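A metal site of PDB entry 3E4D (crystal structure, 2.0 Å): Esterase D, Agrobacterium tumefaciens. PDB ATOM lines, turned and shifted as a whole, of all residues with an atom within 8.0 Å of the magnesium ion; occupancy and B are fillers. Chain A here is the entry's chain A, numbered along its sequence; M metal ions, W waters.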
ATOM      1  N   LEU A  53      15.905 -30.193   6.500  1.00  0.00           N
ATOM      2  CA  LEU A  53      15.390 -29.023   5.791  1.00  0.00           C
ATOM      3  C   LEU A  53      14.149 -28.438   6.454  1.00  0.00           C
ATOM      4  O   LEU A  53      13.234 -29.185   6.858  1.00  0.00           O
ATOM      5  CB  LEU A  53      15.083 -29.361   4.323  1.00  0.00           C
ATOM      6  CG  LEU A  53      16.280 -29.440   3.364  1.00  0.00           C
ATOM      7  CD1 LEU A  53      15.877 -30.116   2.058  1.00  0.00           C
ATOM      8  CD2 LEU A  53      16.851 -28.074   3.119  1.00  0.00           C
ATOM      9  N   THR A  54      14.130 -27.106   6.548  1.00  0.00           N
ATOM     10  CA  THR A  54      13.022 -26.304   7.111  1.00  0.00           C
ATOM     11  C   THR A  54      12.913 -26.299   8.640  1.00  0.00           C
ATOM     12  O   THR A  54      12.116 -25.545   9.193  1.00  0.00           O
ATOM     13  CB  THR A  54      11.620 -26.655   6.508  1.00  0.00           C
ATOM     14  OG1 THR A  54      11.100 -27.860   7.111  1.00  0.00           O
ATOM     15  CG2 THR A  54      11.680 -26.814   4.997  1.00  0.00           C
ATOM     16  N   PRO A  90      21.292 -13.847   3.952  1.00  0.00           N
ATOM     17  CA  PRO A  90      20.627 -14.012   2.652  1.00  0.00           C
ATOM     18  C   PRO A  90      19.808 -15.306   2.600  1.00  0.00           C
ATOM     19  O   PRO A  90      20.061 -16.255   3.379  1.00  0.00           O
ATOM     20  CB  PRO A  90      21.789 -14.045   1.649  1.00  0.00           C
ATOM     21  CG  PRO A  90      22.950 -14.524   2.437  1.00  0.00           C
ATOM     22  CD  PRO A  90      22.758 -13.991   3.835  1.00  0.00           C
ATOM     23  N   ASP A  91      18.842 -15.358   1.688  1.00  0.00           N
ATOM     24  CA  ASP A  91      17.924 -16.478   1.611  1.00  0.00           C
ATOM     25  C   ASP A  91      17.532 -16.680   0.168  1.00  0.00           C
ATOM     26  O   ASP A  91      17.696 -15.776  -0.636  1.00  0.00           O
ATOM     27  CB  ASP A  91      16.687 -16.146   2.458  1.00  0.00           C
ATOM     28  CG  ASP A  91      15.771 -17.352   2.698  1.00  0.00           C
ATOM     29  OD1 ASP A  91      16.183 -18.491   2.414  1.00  0.00           O
ATOM     30  OD2 ASP A  91      14.642 -17.131   3.165  1.00  0.00           O
ATOM     31  N   GLU A  92      17.059 -17.873  -0.161  1.00  0.00           N
ATOM     32  CA  GLU A  92      16.276 -18.043  -1.386  1.00  0.00           C
ATOM     33  C   GLU A  92      14.830 -18.243  -0.938  1.00  0.00           C
ATOM     34  O   GLU A  92      14.430 -19.313  -0.510  1.00  0.00           O
ATOM     35  CB  GLU A  92      16.777 -19.194  -2.276  1.00  0.00           C
ATOM     36  CG  GLU A  92      16.399 -18.969  -3.752  1.00  0.00           C
ATOM     37  CD  GLU A  92      16.568 -20.203  -4.636  1.00  0.00           C
ATOM     38  OE1 GLU A  92      17.506 -20.994  -4.404  1.00  0.00           O
ATOM     39  OE2 GLU A  92      15.742 -20.369  -5.580  1.00  0.00           O
ATOM     40  N   LEU A  93      14.058 -17.163  -1.046  1.00  0.00           N
ATOM     41  CA  LEU A  93      12.727 -17.065  -0.445  1.00  0.00           C
ATOM     42  C   LEU A  93      11.708 -18.095  -0.933  1.00  0.00           C
ATOM     43  O   LEU A  93      10.850 -18.540  -0.181  1.00  0.00           O
ATOM     44  CB  LEU A  93      12.172 -15.655  -0.652  1.00  0.00           C
ATOM     45  CG  LEU A  93      10.905 -15.182   0.070  1.00  0.00           C
ATOM     46  CD1 LEU A  93      11.200 -14.783   1.505  1.00  0.00           C
ATOM     47  CD2 LEU A  93      10.324 -14.010  -0.702  1.00  0.00           C
ATOM     48  N   THR A  94      11.780 -18.487  -2.202  1.00  0.00           N
ATOM     49  CA  THR A  94      10.759 -19.355  -2.746  1.00  0.00           C
ATOM     50  C   THR A  94      11.249 -20.781  -2.998  1.00  0.00           C
ATOM     51  O   THR A  94      10.696 -21.501  -3.836  1.00  0.00           O
ATOM     52  CB  THR A  94      10.171 -18.758  -4.026  1.00  0.00           C
ATOM     53  OG1 THR A  94      11.239 -18.424  -4.911  1.00  0.00           O
ATOM     54  CG2 THR A  94       9.343 -17.508  -3.687  1.00  0.00           C
ATOM     55  N   ASN A  95      12.287 -21.159  -2.268  1.00  0.00           N
ATOM     56  CA  ASN A  95      12.809 -22.524  -2.330  1.00  0.00           C
ATOM     57  C   ASN A  95      13.145 -23.004  -0.922  1.00  0.00           C
ATOM     58  O   ASN A  95      14.150 -22.599  -0.343  1.00  0.00           O
ATOM     59  CB  ASN A  95      14.032 -22.577  -3.243  1.00  0.00           C
ATOM     60  CG  ASN A  95      14.491 -23.986  -3.515  1.00  0.00           C
ATOM     61  OD1 ASN A  95      13.961 -24.948  -2.961  1.00  0.00           O
ATOM     62  ND2 ASN A  95      15.489 -24.118  -4.372  1.00  0.00           N
ATOM     63  N   TRP A  96      12.285 -23.859  -0.371  1.00  0.00           N
ATOM     64  CA  TRP A  96      12.518 -24.423   0.962  1.00  0.00           C
ATOM     65  C   TRP A  96      13.764 -25.324   1.012  1.00  0.00           C
ATOM     66  O   TRP A  96      14.230 -25.671   2.091  1.00  0.00           O
ATOM     67  CB  TRP A  96      11.275 -25.172   1.466  1.00  0.00           C
ATOM     68  CG  TRP A  96      10.839 -26.359   0.633  1.00  0.00           C
ATOM     69  CD1 TRP A  96       9.969 -26.338  -0.414  1.00  0.00           C
ATOM     70  CD2 TRP A  96      11.197 -27.748   0.818  1.00  0.00           C
ATOM     71  NE1 TRP A  96       9.775 -27.604  -0.907  1.00  0.00           N
ATOM     72  CE2 TRP A  96      10.523 -28.495  -0.174  1.00  0.00           C
ATOM     73  CE3 TRP A  96      12.038 -28.422   1.719  1.00  0.00           C
ATOM     74  CZ2 TRP A  96      10.641 -29.884  -0.286  1.00  0.00           C
ATOM     75  CZ3 TRP A  96      12.161 -29.807   1.598  1.00  0.00           C
ATOM     76  CH2 TRP A  96      11.475 -30.526   0.604  1.00  0.00           C
ATOM     77  N   GLN A  97      14.297 -25.669  -0.159  1.00  0.00           N
ATOM     78  CA  GLN A  97      15.493 -26.505  -0.283  1.00  0.00           C
ATOM     79  C   GLN A  97      16.794 -25.713  -0.315  1.00  0.00           C
ATOM     80  O   GLN A  97      17.867 -26.282  -0.523  1.00  0.00           O
ATOM     81  CB  GLN A  97      15.375 -27.427  -1.502  1.00  0.00           C
ATOM     82  CG  GLN A  97      14.186 -28.404  -1.432  1.00  0.00           C
ATOM     83  CD  GLN A  97      13.973 -29.226  -2.695  1.00  0.00           C
ATOM     84  OE1 GLN A  97      14.641 -29.028  -3.715  1.00  0.00           O
ATOM     85  NE2 GLN A  97      13.029 -30.155  -2.638  1.00  0.00           N
ATOM     86  N   MET A  98      16.717 -24.395  -0.105  1.00  0.00           N
ATOM     87  CA  MET A  98      17.869 -23.505  -0.187  1.00  0.00           C
ATOM     88  C   MET A  98      17.773 -22.326   0.783  1.00  0.00           C
ATOM     89  O   MET A  98      16.691 -21.788   1.019  1.00  0.00           O
ATOM     90  CB  MET A  98      18.022 -22.971  -1.633  1.00  0.00           C
ATOM     91  CG  MET A  98      19.241 -22.057  -1.846  1.00  0.00           C
ATOM     92  SD  MET A  98      20.955 -22.892  -1.482  1.00  0.00           S
ATOM     93  CE  MET A  98      21.990 -21.307  -1.158  1.00  0.00           C
ATOM     94  N   GLY A  99      18.915 -21.941   1.337  1.00  0.00           N
ATOM     95  CA  GLY A  99      18.979 -20.784   2.212  1.00  0.00           C
ATOM     96  C   GLY A  99      18.684 -21.068   3.672  1.00  0.00           C
ATOM     97  O   GLY A  99      19.293 -21.936   4.286  1.00  0.00           O
ATOM     98  N   LYS A 100      17.758 -20.293   4.230  1.00  0.00           N
ATOM     99  CA  LYS A 100      17.350 -20.457   5.622  1.00  0.00           C
ATOM    100  C   LYS A 100      16.659 -21.801   5.850  1.00  0.00           C
ATOM    101  O   LYS A 100      15.875 -22.274   5.024  1.00  0.00           O
ATOM    102  CB  LYS A 100      16.506 -19.270   6.070  1.00  0.00           C
ATOM    103  CG  LYS A 100      17.320 -17.979   6.197  1.00  0.00           C
ATOM    104  CD  LYS A 100      16.446 -16.792   6.509  1.00  0.00           C
ATOM    105  CE  LYS A 100      17.275 -15.527   6.601  1.00  0.00           C
ATOM    106  NZ  LYS A 100      16.443 -14.331   6.930  1.00  0.00           N
ATOM    107  N   GLY A 101      16.990 -22.425   6.977  1.00  0.00           N
ATOM    108  CA  GLY A 101      16.555 -23.796   7.244  1.00  0.00           C
ATOM    109  C   GLY A 101      17.237 -24.808   6.324  1.00  0.00           C
ATOM    110  O   GLY A 101      16.806 -25.954   6.235  1.00  0.00           O
ATOM    111  N   ALA A 102      18.294 -24.382   5.623  1.00  0.00           N
ATOM    112  CA  ALA A 102      18.922 -25.226   4.610  1.00  0.00           C
ATOM    113  C   ALA A 102      20.430 -25.001   4.451  1.00  0.00           C
ATOM    114  O   ALA A 102      20.944 -24.873   3.323  1.00  0.00           O
ATOM    115  CB  ALA A 102      18.200 -25.030   3.258  1.00  0.00           C
ATOM    116  N   TRP A 113      26.544 -16.290   0.325  1.00  0.00           N
ATOM    117  CA  TRP A 113      26.397 -17.329   1.357  1.00  0.00           C
ATOM    118  C   TRP A 113      27.578 -17.457   2.304  1.00  0.00           C
ATOM    119  O   TRP A 113      27.429 -17.887   3.463  1.00  0.00           O
ATOM    120  CB  TRP A 113      26.144 -18.667   0.678  1.00  0.00           C
ATOM    121  CG  TRP A 113      25.186 -18.540  -0.457  1.00  0.00           C
ATOM    122  CD1 TRP A 113      25.470 -18.640  -1.787  1.00  0.00           C
ATOM    123  CD2 TRP A 113      23.783 -18.231  -0.357  1.00  0.00           C
ATOM    124  NE1 TRP A 113      24.332 -18.431  -2.524  1.00  0.00           N
ATOM    125  CE2 TRP A 113      23.284 -18.165  -1.677  1.00  0.00           C
ATOM    126  CE3 TRP A 113      22.902 -17.992   0.716  1.00  0.00           C
ATOM    127  CZ2 TRP A 113      21.934 -17.901  -1.958  1.00  0.00           C
ATOM    128  CZ3 TRP A 113      21.553 -17.727   0.435  1.00  0.00           C
ATOM    129  CH2 TRP A 113      21.083 -17.682  -0.894  1.00  0.00           C
ATOM    130  N   TYR A 117      26.906 -18.628   6.149  1.00  0.00           N
ATOM    131  CA  TYR A 117      26.636 -20.058   6.023  1.00  0.00           C
ATOM    132  C   TYR A 117      27.853 -20.937   6.361  1.00  0.00           C
ATOM    133  O   TYR A 117      28.427 -21.602   5.484  1.00  0.00           O
ATOM    134  CB  TYR A 117      25.990 -20.383   4.671  1.00  0.00           C
ATOM    135  CG  TYR A 117      24.551 -19.909   4.592  1.00  0.00           C
ATOM    136  CD1 TYR A 117      24.235 -18.556   4.382  1.00  0.00           C
ATOM    137  CD2 TYR A 117      23.514 -20.807   4.722  1.00  0.00           C
ATOM    138  CE1 TYR A 117      22.902 -18.122   4.312  1.00  0.00           C
ATOM    139  CE2 TYR A 117      22.189 -20.398   4.668  1.00  0.00           C
ATOM    140  CZ  TYR A 117      21.890 -19.059   4.458  1.00  0.00           C
ATOM    141  OH  TYR A 117      20.576 -18.685   4.400  1.00  0.00           O
ATOM    142  N   TYR A 190      26.258 -22.927  -2.732  1.00  0.00           N
ATOM    143  CA  TYR A 190      27.122 -22.692  -1.576  1.00  0.00           C
ATOM    144  C   TYR A 190      28.592 -22.818  -1.877  1.00  0.00           C
ATOM    145  O   TYR A 190      29.396 -22.063  -1.334  1.00  0.00           O
ATOM    146  CB  TYR A 190      26.787 -23.671  -0.430  1.00  0.00           C
ATOM    147  CG  TYR A 190      25.471 -23.397   0.268  1.00  0.00           C
ATOM    148  CD1 TYR A 190      24.561 -24.431   0.503  1.00  0.00           C
ATOM    149  CD2 TYR A 190      25.133 -22.109   0.678  1.00  0.00           C
ATOM    150  CE1 TYR A 190      23.357 -24.186   1.140  1.00  0.00           C
ATOM    151  CE2 TYR A 190      23.939 -21.860   1.324  1.00  0.00           C
ATOM    152  CZ  TYR A 190      23.055 -22.890   1.551  1.00  0.00           C
ATOM    153  OH  TYR A 190      21.853 -22.616   2.181  1.00  0.00           O
HETATM  154 MG    MG M   1      14.754 -20.984   1.062  1.00  0.00          MG
HETATM  155  O   HOH W   1      14.195 -20.763   3.184  1.00  0.00           O
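The side-chain hydroxyl (OH) of Tyr 190 sits close to the side-chain sulfur (SD) of Met 98. N of Gln 97 is in hydrogen-bond range of OD1 of Asn 95, at 2.9 Å. The side-chain carboxylate of Asp 91 lies within hydrogen-bond range of the backbone NH of Lys 100, at 3.0 Å.
Asp 91 touches the magnesium ion (OD1 to MG, 3.2 Å). Four residues have an atom within 4 Å of the magnesium ion: Asp 91, Glu 92, Asn 95 and Met 98.
O of Met 98 binds the magnesium ion, at 2.1 Å. The magnesium ion is bound by water W1 (2.2 Å). The magnesium ion is bound by O of Asn 95 (2.2 Å). The backbone carbonyl oxygen (O) of Glu 92 binds the magnesium ion (2.3 Å).
Water W1 bridges the backbone carbonyl oxygen (O) of Lys 100 and the side-chain carboxylate (OD1) of Asp 91.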
